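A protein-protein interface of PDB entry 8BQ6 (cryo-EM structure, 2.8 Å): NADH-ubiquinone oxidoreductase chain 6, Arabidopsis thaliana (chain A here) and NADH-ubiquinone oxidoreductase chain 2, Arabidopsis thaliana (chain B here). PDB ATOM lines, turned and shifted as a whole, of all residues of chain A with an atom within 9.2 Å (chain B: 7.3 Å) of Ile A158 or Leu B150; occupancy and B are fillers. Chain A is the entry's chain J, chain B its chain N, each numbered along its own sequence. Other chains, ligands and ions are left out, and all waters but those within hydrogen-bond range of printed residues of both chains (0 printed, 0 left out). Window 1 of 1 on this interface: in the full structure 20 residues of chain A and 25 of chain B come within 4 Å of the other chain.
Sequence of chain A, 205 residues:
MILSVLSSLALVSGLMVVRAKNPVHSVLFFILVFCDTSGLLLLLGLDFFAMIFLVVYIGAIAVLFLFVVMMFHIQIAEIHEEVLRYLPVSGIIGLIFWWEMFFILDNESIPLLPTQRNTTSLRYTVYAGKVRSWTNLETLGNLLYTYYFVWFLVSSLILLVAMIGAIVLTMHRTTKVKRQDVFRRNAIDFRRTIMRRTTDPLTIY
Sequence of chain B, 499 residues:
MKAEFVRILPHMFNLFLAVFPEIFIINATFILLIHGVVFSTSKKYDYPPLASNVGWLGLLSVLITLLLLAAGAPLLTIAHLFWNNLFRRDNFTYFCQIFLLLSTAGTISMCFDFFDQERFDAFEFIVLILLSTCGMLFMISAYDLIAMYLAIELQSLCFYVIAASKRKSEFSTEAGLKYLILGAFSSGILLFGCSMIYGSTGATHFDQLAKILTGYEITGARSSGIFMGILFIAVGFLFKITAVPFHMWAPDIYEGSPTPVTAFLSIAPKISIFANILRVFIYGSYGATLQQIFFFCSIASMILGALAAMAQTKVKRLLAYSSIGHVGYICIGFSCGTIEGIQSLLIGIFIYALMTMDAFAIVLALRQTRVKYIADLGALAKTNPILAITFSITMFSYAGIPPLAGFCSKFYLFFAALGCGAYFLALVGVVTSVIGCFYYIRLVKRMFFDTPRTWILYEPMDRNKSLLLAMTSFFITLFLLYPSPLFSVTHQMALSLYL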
ATOM      1  N   TYR A 148     -26.290 -27.118 -11.536  1.00  0.00           N
ATOM      2  CA  TYR A 148     -26.341 -27.436 -10.119  1.00  0.00           C
ATOM      3  C   TYR A 148     -25.728 -26.315  -9.288  1.00  0.00           C
ATOM      4  O   TYR A 148     -25.043 -26.560  -8.293  1.00  0.00           O
ATOM      5  CB  TYR A 148     -25.668 -28.782  -9.858  1.00  0.00           C
ATOM      6  CG  TYR A 148     -26.376 -29.905 -10.583  1.00  0.00           C
ATOM      7  CD1 TYR A 148     -27.482 -30.516 -10.018  1.00  0.00           C
ATOM      8  CD2 TYR A 148     -25.969 -30.328 -11.844  1.00  0.00           C
ATOM      9  CE1 TYR A 148     -28.152 -31.523 -10.668  1.00  0.00           C
ATOM     10  CE2 TYR A 148     -26.640 -31.341 -12.506  1.00  0.00           C
ATOM     11  CZ  TYR A 148     -27.733 -31.933 -11.909  1.00  0.00           C
ATOM     12  OH  TYR A 148     -28.419 -32.944 -12.539  1.00  0.00           O
ATOM     13  N   PHE A 149     -26.014 -25.060  -9.655  1.00  0.00           N
ATOM     14  CA  PHE A 149     -25.335 -23.921  -9.035  1.00  0.00           C
ATOM     15  C   PHE A 149     -25.826 -23.650  -7.614  1.00  0.00           C
ATOM     16  O   PHE A 149     -25.092 -23.060  -6.806  1.00  0.00           O
ATOM     17  CB  PHE A 149     -25.500 -22.672  -9.910  1.00  0.00           C
ATOM     18  CG  PHE A 149     -26.848 -22.012  -9.791  1.00  0.00           C
ATOM     19  CD1 PHE A 149     -27.925 -22.466 -10.535  1.00  0.00           C
ATOM     20  CD2 PHE A 149     -27.035 -20.935  -8.940  1.00  0.00           C
ATOM     21  CE1 PHE A 149     -29.163 -21.870 -10.424  1.00  0.00           C
ATOM     22  CE2 PHE A 149     -28.273 -20.335  -8.824  1.00  0.00           C
ATOM     23  CZ  PHE A 149     -29.338 -20.802  -9.570  1.00  0.00           C
ATOM     24  N   VAL A 150     -27.053 -24.060  -7.288  1.00  0.00           N
ATOM     25  CA  VAL A 150     -27.600 -23.794  -5.961  1.00  0.00           C
ATOM     26  C   VAL A 150     -26.813 -24.544  -4.894  1.00  0.00           C
ATOM     27  O   VAL A 150     -26.554 -24.016  -3.806  1.00  0.00           O
ATOM     28  CB  VAL A 150     -29.098 -24.151  -5.923  1.00  0.00           C
ATOM     29  CG1 VAL A 150     -29.584 -24.302  -4.489  1.00  0.00           C
ATOM     30  CG2 VAL A 150     -29.911 -23.102  -6.662  1.00  0.00           C
ATOM     31  N   TRP A 151     -26.437 -25.793  -5.178  1.00  0.00           N
ATOM     32  CA  TRP A 151     -25.669 -26.577  -4.214  1.00  0.00           C
ATOM     33  C   TRP A 151     -24.272 -26.006  -4.027  1.00  0.00           C
ATOM     34  O   TRP A 151     -23.729 -26.001  -2.916  1.00  0.00           O
ATOM     35  CB  TRP A 151     -25.595 -28.029  -4.671  1.00  0.00           C
ATOM     36  CG  TRP A 151     -26.919 -28.636  -4.937  1.00  0.00           C
ATOM     37  CD1 TRP A 151     -28.129 -28.185  -4.508  1.00  0.00           C
ATOM     38  CD2 TRP A 151     -27.170 -29.845  -5.650  1.00  0.00           C
ATOM     39  NE1 TRP A 151     -29.124 -29.027  -4.932  1.00  0.00           N
ATOM     40  CE2 TRP A 151     -28.560 -30.059  -5.634  1.00  0.00           C
ATOM     41  CE3 TRP A 151     -26.355 -30.766  -6.310  1.00  0.00           C
ATOM     42  CZ2 TRP A 151     -29.151 -31.152  -6.250  1.00  0.00           C
ATOM     43  CZ3 TRP A 151     -26.941 -31.848  -6.918  1.00  0.00           C
ATOM     44  CH2 TRP A 151     -28.326 -32.035  -6.888  1.00  0.00           C
ATOM     45  N   PHE A 152     -23.676 -25.544  -5.120  1.00  0.00           N
ATOM     46  CA  PHE A 152     -22.451 -24.758  -5.078  1.00  0.00           C
ATOM     47  C   PHE A 152     -22.570 -23.589  -4.091  1.00  0.00           C
ATOM     48  O   PHE A 152     -21.710 -23.386  -3.218  1.00  0.00           O
ATOM     49  CB  PHE A 152     -22.190 -24.286  -6.510  1.00  0.00           C
ATOM     50  CG  PHE A 152     -20.975 -23.460  -6.685  1.00  0.00           C
ATOM     51  CD1 PHE A 152     -19.755 -23.879  -6.205  1.00  0.00           C
ATOM     52  CD2 PHE A 152     -21.054 -22.260  -7.363  1.00  0.00           C
ATOM     53  CE1 PHE A 152     -18.639 -23.109  -6.388  1.00  0.00           C
ATOM     54  CE2 PHE A 152     -19.944 -21.488  -7.544  1.00  0.00           C
ATOM     55  CZ  PHE A 152     -18.733 -21.912  -7.059  1.00  0.00           C
ATOM     56  N   LEU A 153     -23.665 -22.832  -4.188  1.00  0.00           N
ATOM     57  CA  LEU A 153     -23.827 -21.673  -3.311  1.00  0.00           C
ATOM     58  C   LEU A 153     -24.088 -22.080  -1.858  1.00  0.00           C
ATOM     59  O   LEU A 153     -23.619 -21.413  -0.922  1.00  0.00           O
ATOM     60  CB  LEU A 153     -24.943 -20.780  -3.840  1.00  0.00           C
ATOM     61  CG  LEU A 153     -24.630 -20.153  -5.198  1.00  0.00           C
ATOM     62  CD1 LEU A 153     -25.758 -19.251  -5.639  1.00  0.00           C
ATOM     63  CD2 LEU A 153     -23.317 -19.386  -5.134  1.00  0.00           C
ATOM     64  N   VAL A 154     -24.838 -23.163  -1.643  1.00  0.00           N
ATOM     65  CA  VAL A 154     -25.051 -23.651  -0.281  1.00  0.00           C
ATOM     66  C   VAL A 154     -23.723 -24.071   0.345  1.00  0.00           C
ATOM     67  O   VAL A 154     -23.488 -23.868   1.546  1.00  0.00           O
ATOM     68  CB  VAL A 154     -26.074 -24.802  -0.272  1.00  0.00           C
ATOM     69  CG1 VAL A 154     -26.157 -25.428   1.107  1.00  0.00           C
ATOM     70  CG2 VAL A 154     -27.441 -24.304  -0.697  1.00  0.00           C
ATOM     71  N   SER A 155     -22.835 -24.664  -0.456  1.00  0.00           N
ATOM     72  CA  SER A 155     -21.509 -25.002   0.051  1.00  0.00           C
ATOM     73  C   SER A 155     -20.729 -23.747   0.436  1.00  0.00           C
ATOM     74  O   SER A 155     -19.985 -23.745   1.428  1.00  0.00           O
ATOM     75  CB  SER A 155     -20.747 -25.833  -0.985  1.00  0.00           C
ATOM     76  OG  SER A 155     -20.088 -25.019  -1.937  1.00  0.00           O
ATOM     77  N   SER A 156     -20.885 -22.668  -0.336  1.00  0.00           N
ATOM     78  CA  SER A 156     -20.288 -21.399   0.087  1.00  0.00           C
ATOM     79  C   SER A 156     -20.831 -20.949   1.443  1.00  0.00           C
ATOM     80  O   SER A 156     -20.085 -20.424   2.279  1.00  0.00           O
ATOM     81  CB  SER A 156     -20.527 -20.317  -0.962  1.00  0.00           C
ATOM     82  OG  SER A 156     -21.794 -19.711  -0.802  1.00  0.00           O
ATOM     83  N   LEU A 157     -22.135 -21.125   1.669  1.00  0.00           N
ATOM     84  CA  LEU A 157     -22.704 -20.763   2.969  1.00  0.00           C
ATOM     85  C   LEU A 157     -22.090 -21.597   4.092  1.00  0.00           C
ATOM     86  O   LEU A 157     -21.828 -21.091   5.194  1.00  0.00           O
ATOM     87  CB  LEU A 157     -24.220 -20.930   2.940  1.00  0.00           C
ATOM     88  CG  LEU A 157     -24.970 -19.824   2.203  1.00  0.00           C
ATOM     89  CD1 LEU A 157     -26.461 -20.046   2.316  1.00  0.00           C
ATOM     90  CD2 LEU A 157     -24.587 -18.465   2.757  1.00  0.00           C
ATOM     91  N   ILE A 158     -21.851 -22.880   3.820  1.00  0.00           N
ATOM     92  CA  ILE A 158     -21.181 -23.756   4.782  1.00  0.00           C
ATOM     93  C   ILE A 158     -19.780 -23.232   5.112  1.00  0.00           C
ATOM     94  O   ILE A 158     -19.368 -23.184   6.285  1.00  0.00           O
ATOM     95  CB  ILE A 158     -21.159 -25.193   4.225  1.00  0.00           C
ATOM     96  CG1 ILE A 158     -22.508 -25.878   4.467  1.00  0.00           C
ATOM     97  CG2 ILE A 158     -20.023 -26.000   4.807  1.00  0.00           C
ATOM     98  CD1 ILE A 158     -22.768 -27.060   3.564  1.00  0.00           C
ATOM     99  N   LEU A 159     -19.031 -22.817   4.089  1.00  0.00           N
ATOM    100  CA  LEU A 159     -17.695 -22.272   4.337  1.00  0.00           C
ATOM    101  C   LEU A 159     -17.754 -20.977   5.147  1.00  0.00           C
ATOM    102  O   LEU A 159     -16.924 -20.753   6.042  1.00  0.00           O
ATOM    103  CB  LEU A 159     -16.962 -22.049   3.016  1.00  0.00           C
ATOM    104  CG  LEU A 159     -16.566 -23.322   2.268  1.00  0.00           C
ATOM    105  CD1 LEU A 159     -15.937 -22.972   0.937  1.00  0.00           C
ATOM    106  CD2 LEU A 159     -15.620 -24.158   3.109  1.00  0.00           C
ATOM    107  N   LEU A 160     -18.723 -20.109   4.840  1.00  0.00           N
ATOM    108  CA  LEU A 160     -18.904 -18.884   5.618  1.00  0.00           C
ATOM    109  C   LEU A 160     -19.148 -19.196   7.089  1.00  0.00           C
ATOM    110  O   LEU A 160     -18.591 -18.531   7.976  1.00  0.00           O
ATOM    111  CB  LEU A 160     -20.066 -18.065   5.054  1.00  0.00           C
ATOM    112  CG  LEU A 160     -20.447 -16.759   5.766  1.00  0.00           C
ATOM    113  CD1 LEU A 160     -19.261 -15.837   5.943  1.00  0.00           C
ATOM    114  CD2 LEU A 160     -21.578 -16.045   5.054  1.00  0.00           C
ATOM    115  N   VAL A 161     -19.988 -20.196   7.367  1.00  0.00           N
ATOM    116  CA  VAL A 161     -20.226 -20.582   8.756  1.00  0.00           C
ATOM    117  C   VAL A 161     -18.928 -21.036   9.411  1.00  0.00           C
ATOM    118  O   VAL A 161     -18.665 -20.720  10.577  1.00  0.00           O
ATOM    119  CB  VAL A 161     -21.315 -21.666   8.845  1.00  0.00           C
ATOM    120  CG1 VAL A 161     -21.394 -22.225  10.260  1.00  0.00           C
ATOM    121  CG2 VAL A 161     -22.652 -21.092   8.436  1.00  0.00           C
ATOM    122  N   ALA A 162     -18.099 -21.787   8.682  1.00  0.00           N
ATOM    123  CA  ALA A 162     -16.831 -22.221   9.267  1.00  0.00           C
ATOM    124  C   ALA A 162     -15.947 -21.028   9.638  1.00  0.00           C
ATOM    125  O   ALA A 162     -15.356 -20.997  10.723  1.00  0.00           O
ATOM    126  CB  ALA A 162     -16.100 -23.169   8.317  1.00  0.00           C
ATOM    127  N   MET A 163     -15.859 -20.026   8.755  1.00  0.00           N
ATOM    128  CA  MET A 163     -15.028 -18.852   9.054  1.00  0.00           C
ATOM    129  C   MET A 163     -15.553 -18.092  10.271  1.00  0.00           C
ATOM    130  O   MET A 163     -14.787 -17.723  11.181  1.00  0.00           O
ATOM    131  CB  MET A 163     -14.955 -17.926   7.838  1.00  0.00           C
ATOM    132  CG  MET A 163     -14.747 -18.661   6.533  1.00  0.00           C
ATOM    133  SD  MET A 163     -14.990 -17.716   5.014  1.00  0.00           S
ATOM    134  CE  MET A 163     -13.755 -16.444   5.185  1.00  0.00           C
ATOM    135  N   ILE A 164     -16.867 -17.862  10.308  1.00  0.00           N
ATOM    136  CA  ILE A 164     -17.462 -17.133  11.423  1.00  0.00           C
ATOM    137  C   ILE A 164     -17.225 -17.880  12.727  1.00  0.00           C
ATOM    138  O   ILE A 164     -16.769 -17.301  13.719  1.00  0.00           O
ATOM    139  CB  ILE A 164     -18.964 -16.910  11.175  1.00  0.00           C
ATOM    140  CG1 ILE A 164     -19.177 -15.692  10.284  1.00  0.00           C
ATOM    141  CG2 ILE A 164     -19.700 -16.725  12.492  1.00  0.00           C
ATOM    142  CD1 ILE A 164     -20.587 -15.569   9.778  1.00  0.00           C
ATOM    143  N   GLY A 165     -17.531 -19.180  12.738  1.00  0.00           N
ATOM    144  CA  GLY A 165     -17.417 -19.957  13.959  1.00  0.00           C
ATOM    145  C   GLY A 165     -15.989 -20.087  14.448  1.00  0.00           C
ATOM    146  O   GLY A 165     -15.737 -20.082  15.656  1.00  0.00           O
ATOM    147  N   ALA A 166     -15.032 -20.206  13.520  1.00  0.00           N
ATOM    148  CA  ALA A 166     -13.630 -20.216  13.918  1.00  0.00           C
ATOM    149  C   ALA A 166     -13.254 -18.920  14.615  1.00  0.00           C
ATOM    150  O   ALA A 166     -12.615 -18.946  15.672  1.00  0.00           O
ATOM    151  CB  ALA A 166     -12.729 -20.444  12.706  1.00  0.00           C
ATOM    152  N   GLY B 135     -30.612 -22.806   6.259  1.00  0.00           N
ATOM    153  CA  GLY B 135     -30.329 -24.213   6.028  1.00  0.00           C
ATOM    154  C   GLY B 135     -31.547 -25.099   6.208  1.00  0.00           C
ATOM    155  O   GLY B 135     -31.758 -26.042   5.447  1.00  0.00           O
ATOM    156  N   PHE B 138     -33.898 -24.663   3.266  1.00  0.00           N
ATOM    157  CA  PHE B 138     -33.462 -25.494   2.150  1.00  0.00           C
ATOM    158  C   PHE B 138     -33.671 -26.975   2.440  1.00  0.00           C
ATOM    159  O   PHE B 138     -33.900 -27.755   1.511  1.00  0.00           O
ATOM    160  CB  PHE B 138     -32.001 -25.204   1.814  1.00  0.00           C
ATOM    161  CG  PHE B 138     -31.817 -23.960   1.002  1.00  0.00           C
ATOM    162  CD1 PHE B 138     -32.346 -23.871  -0.272  1.00  0.00           C
ATOM    163  CD2 PHE B 138     -31.141 -22.871   1.518  1.00  0.00           C
ATOM    164  CE1 PHE B 138     -32.195 -22.725  -1.022  1.00  0.00           C
ATOM    165  CE2 PHE B 138     -30.986 -21.721   0.771  1.00  0.00           C
ATOM    166  CZ  PHE B 138     -31.514 -21.649  -0.499  1.00  0.00           C
ATOM    167  N   MET B 139     -33.604 -27.378   3.712  1.00  0.00           N
ATOM    168  CA  MET B 139     -33.867 -28.770   4.064  1.00  0.00           C
ATOM    169  C   MET B 139     -35.287 -29.161   3.686  1.00  0.00           C
ATOM    170  O   MET B 139     -35.523 -30.251   3.152  1.00  0.00           O
ATOM    171  CB  MET B 139     -33.656 -29.003   5.561  1.00  0.00           C
ATOM    172  CG  MET B 139     -32.245 -29.396   5.931  1.00  0.00           C
ATOM    173  SD  MET B 139     -31.825 -29.442   7.675  1.00  0.00           S
ATOM    174  CE  MET B 139     -33.220 -30.343   8.304  1.00  0.00           C
ATOM    175  N   ASP B 144     -33.534 -34.239  -3.308  1.00  0.00           N
ATOM    176  CA  ASP B 144     -32.421 -35.008  -3.831  1.00  0.00           C
ATOM    177  C   ASP B 144     -31.522 -35.294  -2.643  1.00  0.00           C
ATOM    178  O   ASP B 144     -31.413 -34.469  -1.733  1.00  0.00           O
ATOM    179  CB  ASP B 144     -31.695 -34.226  -4.937  1.00  0.00           C
ATOM    180  CG  ASP B 144     -30.468 -34.941  -5.490  1.00  0.00           C
ATOM    181  OD1 ASP B 144     -29.679 -35.532  -4.724  1.00  0.00           O
ATOM    182  OD2 ASP B 144     -30.284 -34.892  -6.722  1.00  0.00           O
ATOM    183  N   LEU B 145     -30.893 -36.469  -2.645  1.00  0.00           N
ATOM    184  CA  LEU B 145     -30.061 -36.836  -1.505  1.00  0.00           C
ATOM    185  C   LEU B 145     -28.927 -35.836  -1.310  1.00  0.00           C
ATOM    186  O   LEU B 145     -28.572 -35.500  -0.173  1.00  0.00           O
ATOM    187  CB  LEU B 145     -29.498 -38.241  -1.685  1.00  0.00           C
ATOM    188  CG  LEU B 145     -30.486 -39.395  -1.828  1.00  0.00           C
ATOM    189  CD1 LEU B 145     -29.840 -40.486  -2.655  1.00  0.00           C
ATOM    190  CD2 LEU B 145     -30.949 -39.919  -0.483  1.00  0.00           C
ATOM    191  N   ILE B 146     -28.359 -35.342  -2.410  1.00  0.00           N
ATOM    192  CA  ILE B 146     -27.249 -34.396  -2.329  1.00  0.00           C
ATOM    193  C   ILE B 146     -27.689 -33.116  -1.630  1.00  0.00           C
ATOM    194  O   ILE B 146     -27.046 -32.646  -0.679  1.00  0.00           O
ATOM    195  CB  ILE B 146     -26.704 -34.104  -3.736  1.00  0.00           C
ATOM    196  CG1 ILE B 146     -26.187 -35.390  -4.385  1.00  0.00           C
ATOM    197  CG2 ILE B 146     -25.623 -33.035  -3.677  1.00  0.00           C
ATOM    198  CD1 ILE B 146     -25.946 -35.274  -5.873  1.00  0.00           C
ATOM    199  N   ALA B 147     -28.798 -32.533  -2.093  1.00  0.00           N
ATOM    200  CA  ALA B 147     -29.287 -31.291  -1.506  1.00  0.00           C
ATOM    201  C   ALA B 147     -29.690 -31.499  -0.055  1.00  0.00           C
ATOM    202  O   ALA B 147     -29.435 -30.644   0.805  1.00  0.00           O
ATOM    203  CB  ALA B 147     -30.465 -30.759  -2.321  1.00  0.00           C
ATOM    204  N   MET B 148     -30.323 -32.638   0.227  1.00  0.00           N
ATOM    205  CA  MET B 148     -30.699 -32.980   1.591  1.00  0.00           C
ATOM    206  C   MET B 148     -29.483 -32.971   2.509  1.00  0.00           C
ATOM    207  O   MET B 148     -29.492 -32.327   3.567  1.00  0.00           O
ATOM    208  CB  MET B 148     -31.381 -34.348   1.591  1.00  0.00           C
ATOM    209  CG  MET B 148     -31.959 -34.787   2.917  1.00  0.00           C
ATOM    210  SD  MET B 148     -32.222 -36.571   2.998  1.00  0.00           S
ATOM    211  CE  MET B 148     -30.618 -37.196   2.508  1.00  0.00           C
ATOM    212  N   TYR B 149     -28.416 -33.661   2.103  1.00  0.00           N
ATOM    213  CA  TYR B 149     -27.215 -33.724   2.929  1.00  0.00           C
ATOM    214  C   TYR B 149     -26.592 -32.350   3.113  1.00  0.00           C
ATOM    215  O   TYR B 149     -26.160 -32.002   4.218  1.00  0.00           O
ATOM    216  CB  TYR B 149     -26.200 -34.683   2.316  1.00  0.00           C
ATOM    217  CG  TYR B 149     -24.855 -34.653   3.001  1.00  0.00           C
ATOM    218  CD1 TYR B 149     -24.667 -35.265   4.230  1.00  0.00           C
ATOM    219  CD2 TYR B 149     -23.775 -34.015   2.416  1.00  0.00           C
ATOM    220  CE1 TYR B 149     -23.441 -35.242   4.856  1.00  0.00           C
ATOM    221  CE2 TYR B 149     -22.548 -33.986   3.034  1.00  0.00           C
ATOM    222  CZ  TYR B 149     -22.385 -34.601   4.251  1.00  0.00           C
ATOM    223  OH  TYR B 149     -21.158 -34.572   4.867  1.00  0.00           O
ATOM    224  N   LEU B 150     -26.511 -31.561   2.041  1.00  0.00           N
ATOM    225  CA  LEU B 150     -25.898 -30.241   2.160  1.00  0.00           C
ATOM    226  C   LEU B 150     -26.655 -29.368   3.153  1.00  0.00           C
ATOM    227  O   LEU B 150     -26.052 -28.734   4.030  1.00  0.00           O
ATOM    228  CB  LEU B 150     -25.826 -29.572   0.789  1.00  0.00           C
ATOM    229  CG  LEU B 150     -24.795 -30.175  -0.162  1.00  0.00           C
ATOM    230  CD1 LEU B 150     -24.519 -29.230  -1.303  1.00  0.00           C
ATOM    231  CD2 LEU B 150     -23.505 -30.455   0.596  1.00  0.00           C
ATOM    232  N   ALA B 151     -27.982 -29.327   3.033  1.00  0.00           N
ATOM    233  CA  ALA B 151     -28.773 -28.492   3.931  1.00  0.00           C
ATOM    234  C   ALA B 151     -28.669 -28.983   5.372  1.00  0.00           C
ATOM    235  O   ALA B 151     -28.569 -28.176   6.313  1.00  0.00           O
ATOM    236  CB  ALA B 151     -30.220 -28.461   3.451  1.00  0.00           C
ATOM    237  N   ILE B 152     -28.657 -30.305   5.557  1.00  0.00           N
ATOM    238  CA  ILE B 152     -28.496 -30.878   6.888  1.00  0.00           C
ATOM    239  C   ILE B 152     -27.157 -30.466   7.487  1.00  0.00           C
ATOM    240  O   ILE B 152     -27.077 -30.093   8.664  1.00  0.00           O
ATOM    241  CB  ILE B 152     -28.649 -32.407   6.810  1.00  0.00           C
ATOM    242  CG1 ILE B 152     -30.112 -32.768   6.567  1.00  0.00           C
ATOM    243  CG2 ILE B 152     -28.166 -33.063   8.083  1.00  0.00           C
ATOM    244  CD1 ILE B 152     -30.360 -34.243   6.427  1.00  0.00           C
ATOM    245  N   GLU B 153     -26.089 -30.510   6.685  1.00  0.00           N
ATOM    246  CA  GLU B 153     -24.765 -30.138   7.178  1.00  0.00           C
ATOM    247  C   GLU B 153     -24.685 -28.661   7.534  1.00  0.00           C
ATOM    248  O   GLU B 153     -24.043 -28.296   8.524  1.00  0.00           O
ATOM    249  CB  GLU B 153     -23.691 -30.481   6.150  1.00  0.00           C
ATOM    250  CG  GLU B 153     -23.440 -31.956   5.997  1.00  0.00           C
ATOM    251  CD  GLU B 153     -23.405 -32.685   7.326  1.00  0.00           C
ATOM    252  OE1 GLU B 153     -22.376 -32.609   8.027  1.00  0.00           O
ATOM    253  OE2 GLU B 153     -24.411 -33.341   7.668  1.00  0.00           O
ATOM    254  N   LEU B 154     -25.289 -27.793   6.723  1.00  0.00           N
ATOM    255  CA  LEU B 154     -25.279 -26.367   7.045  1.00  0.00           C
ATOM    256  C   LEU B 154     -25.955 -26.114   8.389  1.00  0.00           C
ATOM    257  O   LEU B 154     -25.399 -25.440   9.279  1.00  0.00           O
ATOM    258  CB  LEU B 154     -25.967 -25.580   5.929  1.00  0.00           C
ATOM    259  CG  LEU B 154     -26.280 -24.102   6.174  1.00  0.00           C
ATOM    260  CD1 LEU B 154     -25.040 -23.343   6.604  1.00  0.00           C
ATOM    261  CD2 LEU B 154     -26.887 -23.470   4.934  1.00  0.00           C
ATOM    262  N   GLN B 155     -27.144 -26.691   8.565  1.00  0.00           N
ATOM    263  CA  GLN B 155     -27.858 -26.551   9.826  1.00  0.00           C
ATOM    264  C   GLN B 155     -27.030 -27.091  10.993  1.00  0.00           C
ATOM    265  O   GLN B 155     -26.891 -26.434  12.038  1.00  0.00           O
ATOM    266  CB  GLN B 155     -29.202 -27.262   9.695  1.00  0.00           C
ATOM    267  CG  GLN B 155     -30.023 -27.323  10.925  1.00  0.00           C
ATOM    268  CD  GLN B 155     -30.306 -28.744  11.312  1.00  0.00           C
ATOM    269  OE1 GLN B 155     -29.393 -29.500  11.639  1.00  0.00           O
ATOM    270  NE2 GLN B 155     -31.573 -29.131  11.256  1.00  0.00           N
ATOM    271  N   SER B 156     -26.421 -28.267  10.807  1.00  0.00           N
ATOM    272  CA  SER B 156     -25.656 -28.909  11.872  1.00  0.00           C
ATOM    273  C   SER B 156     -24.432 -28.094  12.270  1.00  0.00           C
ATOM    274  O   SER B 156     -24.104 -28.002  13.457  1.00  0.00           O
ATOM    275  CB  SER B 156     -25.231 -30.308  11.431  1.00  0.00           C
ATOM    276  OG  SER B 156     -26.281 -31.239  11.598  1.00  0.00           O
ATOM    277  N   LEU B 157     -23.716 -27.533  11.293  1.00  0.00           N
ATOM    278  CA  LEU B 157     -22.531 -26.741  11.609  1.00  0.00           C
ATOM    279  C   LEU B 157     -22.900 -25.492  12.396  1.00  0.00           C
ATOM    280  O   LEU B 157     -22.214 -25.129  13.371  1.00  0.00           O
ATOM    281  CB  LEU B 157     -21.793 -26.362  10.328  1.00  0.00           C
ATOM    282  CG  LEU B 157     -21.181 -27.529   9.565  1.00  0.00           C
ATOM    283  CD1 LEU B 157     -20.821 -27.096   8.165  1.00  0.00           C
ATOM    284  CD2 LEU B 157     -19.972 -28.042  10.295  1.00  0.00           C
ATOM    285  N   LEU B 191     -24.255 -40.376   5.042  1.00  0.00           N
ATOM    286  CA  LEU B 191     -23.622 -40.210   3.737  1.00  0.00           C
ATOM    287  C   LEU B 191     -23.255 -41.550   3.117  1.00  0.00           C
ATOM    288  O   LEU B 191     -23.366 -41.734   1.897  1.00  0.00           O
ATOM    289  CB  LEU B 191     -22.377 -39.343   3.873  1.00  0.00           C
ATOM    290  CG  LEU B 191     -22.031 -38.488   2.663  1.00  0.00           C
ATOM    291  CD1 LEU B 191     -23.240 -37.737   2.177  1.00  0.00           C
ATOM    292  CD2 LEU B 191     -20.897 -37.557   3.004  1.00  0.00           C
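OD1 of Asp B144 sits at hydrogen-bond distance from N of Ile B146, 2.7 Å away.
Among the printed residues, merely in contact across the chains: Trp A151 with Asp B144 (3.5 Å), Trp A151 with Ile B146 (3.6 Å), Trp A151 with Ala B147 (3.4 Å), Trp A151 with Leu B150 (3.7 Å), Ile A158 with Leu B150 (3.7 Å), Ile A158 with Leu B154 (3.8 Å), Ile A158 with Leu B157 (3.6 Å) and Val A161 with Leu B154 (3.8 Å).
Ile A158 touches just these residues of chain B: Leu B150 (3.7 Å), Leu B154 (3.8 Å) and Leu B157 (3.6 Å).
Leu B150 touches two residues of chain A.
No residue of chain A comes within 4 Å of Ala B151.
Printed residues of chain A within 4 Å of Ala B147: Trp A151 (3.4 Å).
Of the printed residues of chain A, Asp B144 touches Trp A151.
The nearest residue of chain B that does not touch Ile A158 is Glu B153 (4.4 Å).
The nearest residue of chain A that does not touch Leu B150 is Val A154 (4.2 Å).
Of the 19 printed residues of chain A, 3 touch a printed residue of chain B.
Printed residues of chain A that touch a printed residue of chain B: Trp A151, Ile A158 and Val A161.
Hydrophobic or aromatic side chains of chain A that line the printed part of chain B: Trp A151, Ile A158 and Val A161.
Hydrophobic or aromatic side chains of chain B within 4 Å of the printed part of chain A: Ile B146, Ala B147, Leu B150, Leu B154 and Leu B157.
Along chain B the printed residues that touch a printed residue of chain A span positions 144 to 157.
Among the printed residues, 8 pairs touch across the chains.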
